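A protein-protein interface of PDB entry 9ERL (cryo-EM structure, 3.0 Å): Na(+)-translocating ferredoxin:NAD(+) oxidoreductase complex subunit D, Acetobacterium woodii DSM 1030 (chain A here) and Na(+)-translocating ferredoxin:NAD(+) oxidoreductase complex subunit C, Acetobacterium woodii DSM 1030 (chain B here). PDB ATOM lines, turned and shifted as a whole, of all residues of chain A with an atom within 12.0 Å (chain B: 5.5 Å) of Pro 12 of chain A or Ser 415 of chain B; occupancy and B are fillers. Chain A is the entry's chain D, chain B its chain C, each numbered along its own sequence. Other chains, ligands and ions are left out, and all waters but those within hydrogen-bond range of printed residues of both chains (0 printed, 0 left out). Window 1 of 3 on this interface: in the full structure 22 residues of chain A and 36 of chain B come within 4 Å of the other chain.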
ATOM      1  N   THR A   7     -20.044  25.024 -36.573  1.00  0.00           N
ATOM      2  CA  THR A   7     -19.695  25.524 -35.251  1.00  0.00           C
ATOM      3  C   THR A   7     -18.369  26.268 -35.323  1.00  0.00           C
ATOM      4  O   THR A   7     -17.431  25.819 -35.986  1.00  0.00           O
ATOM      5  CB  THR A   7     -19.600  24.379 -34.239  1.00  0.00           C
ATOM      6  OG1 THR A   7     -20.745  23.528 -34.370  1.00  0.00           O
ATOM      7  CG2 THR A   7     -19.541  24.917 -32.819  1.00  0.00           C
ATOM      8  N   VAL A   8     -18.300  27.413 -34.647  1.00  0.00           N
ATOM      9  CA  VAL A   8     -17.096  28.233 -34.604  1.00  0.00           C
ATOM     10  C   VAL A   8     -16.631  28.329 -33.158  1.00  0.00           C
ATOM     11  O   VAL A   8     -17.433  28.610 -32.260  1.00  0.00           O
ATOM     12  CB  VAL A   8     -17.330  29.631 -35.205  1.00  0.00           C
ATOM     13  CG1 VAL A   8     -17.262  29.567 -36.718  1.00  0.00           C
ATOM     14  CG2 VAL A   8     -18.667  30.194 -34.764  1.00  0.00           C
ATOM     15  N   SER A   9     -15.347  28.081 -32.935  1.00  0.00           N
ATOM     16  CA  SER A   9     -14.755  28.151 -31.606  1.00  0.00           C
ATOM     17  C   SER A   9     -13.264  28.422 -31.767  1.00  0.00           C
ATOM     18  O   SER A   9     -12.789  28.741 -32.862  1.00  0.00           O
ATOM     19  CB  SER A   9     -15.031  26.867 -30.818  1.00  0.00           C
ATOM     20  OG  SER A   9     -14.033  25.891 -31.061  1.00  0.00           O
ATOM     21  N   SER A  10     -12.521  28.294 -30.674  1.00  0.00           N
ATOM     22  CA  SER A  10     -11.086  28.524 -30.663  1.00  0.00           C
ATOM     23  C   SER A  10     -10.339  27.203 -30.528  1.00  0.00           C
ATOM     24  O   SER A  10     -10.904  26.178 -30.138  1.00  0.00           O
ATOM     25  CB  SER A  10     -10.694  29.473 -29.527  1.00  0.00           C
ATOM     26  OG  SER A  10      -9.292  29.482 -29.328  1.00  0.00           O
ATOM     27  N   SER A  11      -9.052  27.242 -30.863  1.00  0.00           N
ATOM     28  CA  SER A  11      -8.214  26.056 -30.806  1.00  0.00           C
ATOM     29  C   SER A  11      -7.955  25.655 -29.353  1.00  0.00           C
ATOM     30  O   SER A  11      -7.990  26.500 -28.455  1.00  0.00           O
ATOM     31  CB  SER A  11      -6.893  26.319 -31.521  1.00  0.00           C
ATOM     32  OG  SER A  11      -7.116  26.670 -32.873  1.00  0.00           O
ATOM     33  N   PRO A  12      -7.694  24.361 -29.086  1.00  0.00           N
ATOM     34  CA  PRO A  12      -7.655  23.204 -29.994  1.00  0.00           C
ATOM     35  C   PRO A  12      -9.043  22.662 -30.302  1.00  0.00           C
ATOM     36  O   PRO A  12     -10.022  23.040 -29.669  1.00  0.00           O
ATOM     37  CB  PRO A  12      -6.814  22.172 -29.216  1.00  0.00           C
ATOM     38  CG  PRO A  12      -6.295  22.881 -27.989  1.00  0.00           C
ATOM     39  CD  PRO A  12      -7.279  23.970 -27.732  1.00  0.00           C
ATOM     40  N   HIS A  13      -9.155  21.766 -31.280  1.00  0.00           N
ATOM     41  CA  HIS A  13     -10.427  21.152 -31.628  1.00  0.00           C
ATOM     42  C   HIS A  13     -10.509  19.691 -31.199  1.00  0.00           C
ATOM     43  O   HIS A  13     -11.472  19.005 -31.554  1.00  0.00           O
ATOM     44  CB  HIS A  13     -10.678  21.288 -33.130  1.00  0.00           C
ATOM     45  CG  HIS A  13     -10.511  22.685 -33.643  1.00  0.00           C
ATOM     46  ND1 HIS A  13     -11.409  23.693 -33.365  1.00  0.00           N
ATOM     47  CD2 HIS A  13      -9.547  23.243 -34.411  1.00  0.00           C
ATOM     48  CE1 HIS A  13     -11.005  24.811 -33.940  1.00  0.00           C
ATOM     49  NE2 HIS A  13      -9.878  24.565 -34.583  1.00  0.00           N
ATOM     50  N   ILE A  14      -9.522  19.199 -30.448  1.00  0.00           N
ATOM     51  CA  ILE A  14      -9.534  17.850 -29.900  1.00  0.00           C
ATOM     52  C   ILE A  14      -9.132  17.914 -28.433  1.00  0.00           C
ATOM     53  O   ILE A  14      -8.442  18.842 -28.000  1.00  0.00           O
ATOM     54  CB  ILE A  14      -8.598  16.895 -30.674  1.00  0.00           C
ATOM     55  CG1 ILE A  14      -7.204  17.507 -30.816  1.00  0.00           C
ATOM     56  CG2 ILE A  14      -9.178  16.561 -32.037  1.00  0.00           C
ATOM     57  CD1 ILE A  14      -6.166  16.537 -31.325  1.00  0.00           C
ATOM     58  N   ARG A  15      -9.568  16.916 -27.664  1.00  0.00           N
ATOM     59  CA  ARG A  15      -9.277  16.838 -26.238  1.00  0.00           C
ATOM     60  C   ARG A  15      -8.853  15.416 -25.893  1.00  0.00           C
ATOM     61  O   ARG A  15      -8.844  14.523 -26.744  1.00  0.00           O
ATOM     62  CB  ARG A  15     -10.485  17.255 -25.390  1.00  0.00           C
ATOM     63  CG  ARG A  15     -10.976  18.670 -25.624  1.00  0.00           C
ATOM     64  CD  ARG A  15     -10.286  19.662 -24.706  1.00  0.00           C
ATOM     65  NE  ARG A  15     -10.897  20.984 -24.774  1.00  0.00           N
ATOM     66  CZ  ARG A  15     -10.716  21.848 -25.763  1.00  0.00           C
ATOM     67  NH1 ARG A  15      -9.945  21.563 -26.798  1.00  0.00           N
ATOM     68  NH2 ARG A  15     -11.327  23.027 -25.714  1.00  0.00           N
ATOM     69  N   ALA A  16      -8.501  15.207 -24.625  1.00  0.00           N
ATOM     70  CA  ALA A  16      -8.148  13.892 -24.118  1.00  0.00           C
ATOM     71  C   ALA A  16      -9.411  13.132 -23.717  1.00  0.00           C
ATOM     72  O   ALA A  16     -10.535  13.538 -24.020  1.00  0.00           O
ATOM     73  CB  ALA A  16      -7.178  14.014 -22.945  1.00  0.00           C
ATOM     74  N   LYS A  17      -9.230  12.007 -23.027  1.00  0.00           N
ATOM     75  CA  LYS A  17     -10.356  11.161 -22.650  1.00  0.00           C
ATOM     76  C   LYS A  17     -10.673  11.184 -21.161  1.00  0.00           C
ATOM     77  O   LYS A  17     -11.827  10.953 -20.788  1.00  0.00           O
ATOM     78  CB  LYS A  17     -10.098   9.716 -23.085  1.00  0.00           C
ATOM     79  CG  LYS A  17     -10.550   9.409 -24.501  1.00  0.00           C
ATOM     80  CD  LYS A  17     -10.918   7.945 -24.659  1.00  0.00           C
ATOM     81  CE  LYS A  17     -10.952   7.540 -26.123  1.00  0.00           C
ATOM     82  NZ  LYS A  17     -11.309   6.104 -26.295  1.00  0.00           N
ATOM     83  N   HIS A  18      -9.692  11.450 -20.306  1.00  0.00           N
ATOM     84  CA  HIS A  18      -9.918  11.424 -18.869  1.00  0.00           C
ATOM     85  C   HIS A  18     -10.689  12.657 -18.411  1.00  0.00           C
ATOM     86  O   HIS A  18     -10.668  13.707 -19.057  1.00  0.00           O
ATOM     87  CB  HIS A  18      -8.588  11.322 -18.119  1.00  0.00           C
ATOM     88  CG  HIS A  18      -7.716  12.530 -18.259  1.00  0.00           C
ATOM     89  ND1 HIS A  18      -6.978  12.788 -19.393  1.00  0.00           N
ATOM     90  CD2 HIS A  18      -7.449  13.540 -17.399  1.00  0.00           C
ATOM     91  CE1 HIS A  18      -6.302  13.911 -19.230  1.00  0.00           C
ATOM     92  NE2 HIS A  18      -6.569  14.387 -18.029  1.00  0.00           N
ATOM     93  N   SER A  19     -11.383  12.513 -17.283  1.00  0.00           N
ATOM     94  CA  SER A  19     -12.167  13.594 -16.695  1.00  0.00           C
ATOM     95  C   SER A  19     -12.135  13.438 -15.177  1.00  0.00           C
ATOM     96  O   SER A  19     -11.377  12.632 -14.632  1.00  0.00           O
ATOM     97  CB  SER A  19     -13.593  13.595 -17.259  1.00  0.00           C
ATOM     98  OG  SER A  19     -14.213  12.334 -17.091  1.00  0.00           O
ATOM     99  N   PRO B 333      -5.647  20.179 -36.475  1.00  0.00           N
ATOM    100  CA  PRO B 333      -6.592  20.168 -35.349  1.00  0.00           C
ATOM    101  C   PRO B 333      -6.127  20.948 -34.133  1.00  0.00           C
ATOM    102  O   PRO B 333      -6.966  21.295 -33.292  1.00  0.00           O
ATOM    103  CB  PRO B 333      -6.727  18.677 -35.022  1.00  0.00           C
ATOM    104  CG  PRO B 333      -5.433  18.089 -35.453  1.00  0.00           C
ATOM    105  CD  PRO B 333      -4.966  18.885 -36.643  1.00  0.00           C
ATOM    106  N   MET B 334      -4.831  21.233 -34.005  1.00  0.00           N
ATOM    107  CA  MET B 334      -4.313  21.916 -32.827  1.00  0.00           C
ATOM    108  C   MET B 334      -4.149  23.417 -33.018  1.00  0.00           C
ATOM    109  O   MET B 334      -4.087  24.146 -32.022  1.00  0.00           O
ATOM    110  CB  MET B 334      -2.963  21.316 -32.415  1.00  0.00           C
ATOM    111  CG  MET B 334      -2.972  19.805 -32.222  1.00  0.00           C
ATOM    112  SD  MET B 334      -3.723  19.252 -30.678  1.00  0.00           S
ATOM    113  CE  MET B 334      -3.057  20.432 -29.513  1.00  0.00           C
ATOM    114  N   ILE B 363     -17.750  18.927 -27.462  1.00  0.00           N
ATOM    115  CA  ILE B 363     -16.915  19.046 -26.273  1.00  0.00           C
ATOM    116  C   ILE B 363     -17.804  19.495 -25.120  1.00  0.00           C
ATOM    117  O   ILE B 363     -18.687  20.341 -25.300  1.00  0.00           O
ATOM    118  CB  ILE B 363     -15.745  20.032 -26.491  1.00  0.00           C
ATOM    119  CG1 ILE B 363     -14.889  19.595 -27.681  1.00  0.00           C
ATOM    120  CG2 ILE B 363     -14.871  20.133 -25.252  1.00  0.00           C
ATOM    121  CD1 ILE B 363     -14.190  20.734 -28.382  1.00  0.00           C
ATOM    122  N   GLY B 412      -1.697  25.187 -27.830  1.00  0.00           N
ATOM    123  CA  GLY B 412      -2.609  24.082 -27.602  1.00  0.00           C
ATOM    124  C   GLY B 412      -2.502  23.422 -26.243  1.00  0.00           C
ATOM    125  O   GLY B 412      -3.214  23.792 -25.308  1.00  0.00           O
ATOM    126  N   SER B 413      -1.599  22.441 -26.144  1.00  0.00           N
ATOM    127  CA  SER B 413      -1.569  21.328 -25.195  1.00  0.00           C
ATOM    128  C   SER B 413      -2.064  21.593 -23.777  1.00  0.00           C
ATOM    129  O   SER B 413      -2.638  20.691 -23.161  1.00  0.00           O
ATOM    130  CB  SER B 413      -0.137  20.791 -25.109  1.00  0.00           C
ATOM    131  OG  SER B 413       0.811  21.830 -25.263  1.00  0.00           O
ATOM    132  N   CYS B 414      -1.806  22.781 -23.225  1.00  0.00           N
ATOM    133  CA  CYS B 414      -2.300  23.091 -21.883  1.00  0.00           C
ATOM    134  C   CYS B 414      -3.817  22.949 -21.798  1.00  0.00           C
ATOM    135  O   CYS B 414      -4.347  22.475 -20.787  1.00  0.00           O
ATOM    136  CB  CYS B 414      -1.870  24.501 -21.473  1.00  0.00           C
ATOM    137  SG  CYS B 414      -2.618  25.844 -22.417  1.00  0.00           S
ATOM    138  N   SER B 415      -4.530  23.345 -22.853  1.00  0.00           N
ATOM    139  CA  SER B 415      -5.977  23.171 -22.910  1.00  0.00           C
ATOM    140  C   SER B 415      -6.386  21.756 -23.293  1.00  0.00           C
ATOM    141  O   SER B 415      -7.536  21.372 -23.060  1.00  0.00           O
ATOM    142  CB  SER B 415      -6.580  24.166 -23.902  1.00  0.00           C
ATOM    143  OG  SER B 415      -7.944  24.403 -23.617  1.00  0.00           O
ATOM    144  N   TYR B 416      -5.473  20.978 -23.877  1.00  0.00           N
ATOM    145  CA  TYR B 416      -5.776  19.627 -24.335  1.00  0.00           C
ATOM    146  C   TYR B 416      -5.826  18.622 -23.188  1.00  0.00           C
ATOM    147  O   TYR B 416      -6.597  17.660 -23.250  1.00  0.00           O
ATOM    148  CB  TYR B 416      -4.734  19.212 -25.378  1.00  0.00           C
ATOM    149  CG  TYR B 416      -4.742  17.758 -25.798  1.00  0.00           C
ATOM    150  CD1 TYR B 416      -5.579  17.314 -26.809  1.00  0.00           C
ATOM    151  CD2 TYR B 416      -3.883  16.839 -25.212  1.00  0.00           C
ATOM    152  CE1 TYR B 416      -5.579  15.993 -27.208  1.00  0.00           C
ATOM    153  CE2 TYR B 416      -3.878  15.516 -25.602  1.00  0.00           C
ATOM    154  CZ  TYR B 416      -4.727  15.099 -26.600  1.00  0.00           C
ATOM    155  OH  TYR B 416      -4.727  13.783 -26.993  1.00  0.00           O
ATOM    156  N   ILE B 417      -5.024  18.830 -22.139  1.00  0.00           N
ATOM    157  CA  ILE B 417      -4.874  17.844 -21.072  1.00  0.00           C
ATOM    158  C   ILE B 417      -5.789  18.108 -19.880  1.00  0.00           C
ATOM    159  O   ILE B 417      -5.816  17.300 -18.942  1.00  0.00           O
ATOM    160  CB  ILE B 417      -3.395  17.789 -20.624  1.00  0.00           C
ATOM    161  CG1 ILE B 417      -3.019  16.393 -20.125  1.00  0.00           C
ATOM    162  CG2 ILE B 417      -3.102  18.854 -19.578  1.00  0.00           C
ATOM    163  CD1 ILE B 417      -2.847  15.379 -21.226  1.00  0.00           C
ATOM    164  N   CYS B 418      -6.555  19.189 -19.897  1.00  0.00           N
ATOM    165  CA  CYS B 418      -7.369  19.567 -18.743  1.00  0.00           C
ATOM    166  C   CYS B 418      -8.512  18.582 -18.532  1.00  0.00           C
ATOM    167  O   CYS B 418      -9.309  18.368 -19.455  1.00  0.00           O
ATOM    168  CB  CYS B 418      -7.919  20.975 -18.935  1.00  0.00           C
ATOM    169  SG  CYS B 418      -8.537  21.748 -17.434  1.00  0.00           S
ATOM    170  N   ARG B 422     -11.459  23.135 -19.841  1.00  0.00           N
ATOM    171  CA  ARG B 422     -11.490  24.588 -19.793  1.00  0.00           C
ATOM    172  C   ARG B 422     -10.900  25.180 -21.073  1.00  0.00           C
ATOM    173  O   ARG B 422     -10.551  24.470 -22.018  1.00  0.00           O
ATOM    174  CB  ARG B 422     -10.756  25.092 -18.554  1.00  0.00           C
ATOM    175  CG  ARG B 422     -11.085  24.311 -17.297  1.00  0.00           C
ATOM    176  CD  ARG B 422     -10.692  25.065 -16.043  1.00  0.00           C
ATOM    177  NE  ARG B 422     -11.762  25.938 -15.582  1.00  0.00           N
ATOM    178  CZ  ARG B 422     -11.579  27.174 -15.141  1.00  0.00           C
ATOM    179  NH1 ARG B 422     -10.373  27.712 -15.071  1.00  0.00           N
ATOM    180  NH2 ARG B 422     -12.635  27.888 -14.759  1.00  0.00           N
ATOM    181  N   THR B 423     -10.780  26.505 -21.095  1.00  0.00           N
ATOM    182  CA  THR B 423     -10.417  27.288 -22.275  1.00  0.00           C
ATOM    183  C   THR B 423      -9.228  28.190 -21.969  1.00  0.00           C
ATOM    184  O   THR B 423      -9.272  29.406 -22.163  1.00  0.00           O
ATOM    185  CB  THR B 423     -11.603  28.112 -22.766  1.00  0.00           C
ATOM    186  OG1 THR B 423     -12.297  28.666 -21.642  1.00  0.00           O
ATOM    187  CG2 THR B 423     -12.563  27.243 -23.559  1.00  0.00           C
ATOM    188  N   LEU B 424      -8.155  27.589 -21.448  1.00  0.00           N
ATOM    189  CA  LEU B 424      -7.030  28.358 -20.917  1.00  0.00           C
ATOM    190  C   LEU B 424      -6.342  29.196 -21.992  1.00  0.00           C
ATOM    191  O   LEU B 424      -5.987  30.358 -21.749  1.00  0.00           O
ATOM    192  CB  LEU B 424      -6.030  27.409 -20.258  1.00  0.00           C
ATOM    193  CG  LEU B 424      -6.635  26.309 -19.383  1.00  0.00           C
ATOM    194  CD1 LEU B 424      -5.578  25.312 -18.960  1.00  0.00           C
ATOM    195  CD2 LEU B 424      -7.307  26.913 -18.169  1.00  0.00           C
ATOM    196  N   VAL B 425      -6.137  28.626 -23.183  1.00  0.00           N
ATOM    197  CA  VAL B 425      -5.396  29.337 -24.221  1.00  0.00           C
ATOM    198  C   VAL B 425      -6.173  30.556 -24.716  1.00  0.00           C
ATOM    199  O   VAL B 425      -5.573  31.587 -25.042  1.00  0.00           O
ATOM    200  CB  VAL B 425      -5.016  28.374 -25.365  1.00  0.00           C
ATOM    201  CG1 VAL B 425      -6.245  27.791 -26.036  1.00  0.00           C
ATOM    202  CG2 VAL B 425      -4.117  29.062 -26.376  1.00  0.00           C
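Of the 14 printed residues of chain B, 7 touch a printed residue of chain A.
The backbone carbonyl oxygen (O) of Pro 333 of chain B lies within hydrogen-bond range of the backbone NH (N) of His 13 of chain A, 3.0 Å away.
A ring nitrogen (NE2) of His 18 of chain A sits at hydrogen-bond distance from the backbone carbonyl oxygen (O) of Ile 417 of chain B (3.1 Å).
O of Tyr 416 of chain B is in hydrogen-bond range of N of Ala 16 of chain A.
The side-chain hydroxyl (OG) of Ser 415 of chain B is in hydrogen-bond range of the backbone carbonyl oxygen (O) of Arg 422 of chain B, at 3.1 Å.
The backbone carbonyl oxygen (O) of Gly 412 of chain B sits close to the side-chain sulfur (SG) of Cys 414 of chain B, 3.6 Å away.
The backbone carbonyl oxygen (O) of Pro 12 of chain A sits at hydrogen-bond distance from the guanidinium group (NH1) of Arg 15 of chain A (3.2 Å).
Among the printed residues, merely in contact across the chains: Ser 11 of chain A with Val 425 of chain B, Ile 14 of chain A with Tyr 416 of chain B, Arg 15 of chain A with Tyr 416 of chain B, Ser 11 of chain A with Met 334 of chain B, Arg 15 of chain A with Ser 415 of chain B, Ile 14 of chain A with Met 334 of chain B, Pro 12 of chain A with Pro 333 of chain B, Pro 12 of chain A with Gly 412 of chain B and Pro 12 of chain A with Ser 415 of chain B.
Of the printed residues of chain B, Ile 14 of chain A touches Met 334 and Tyr 416.
Printed residues of chain A within 4 Å of Pro 333 of chain B: Pro 12 and His 13.
Met 334 of chain B touches just these residues of chain A: Ser 11 (3.6 Å) and Ile 14 (3.7 Å).
Gly 412 of chain B touches just one residue of chain A: Pro 12.
No residue of chain A comes within 4 Å of Ser 413 of chain B.
No residue of chain A comes within 4 Å of Cys 414 of chain B.
Ile 417 of chain B touches just one residue of chain A: His 18.
No residue of chain A comes within 4 Å of Cys 418 of chain B.
No residue of chain A comes within 4 Å of Thr 423 of chain B.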
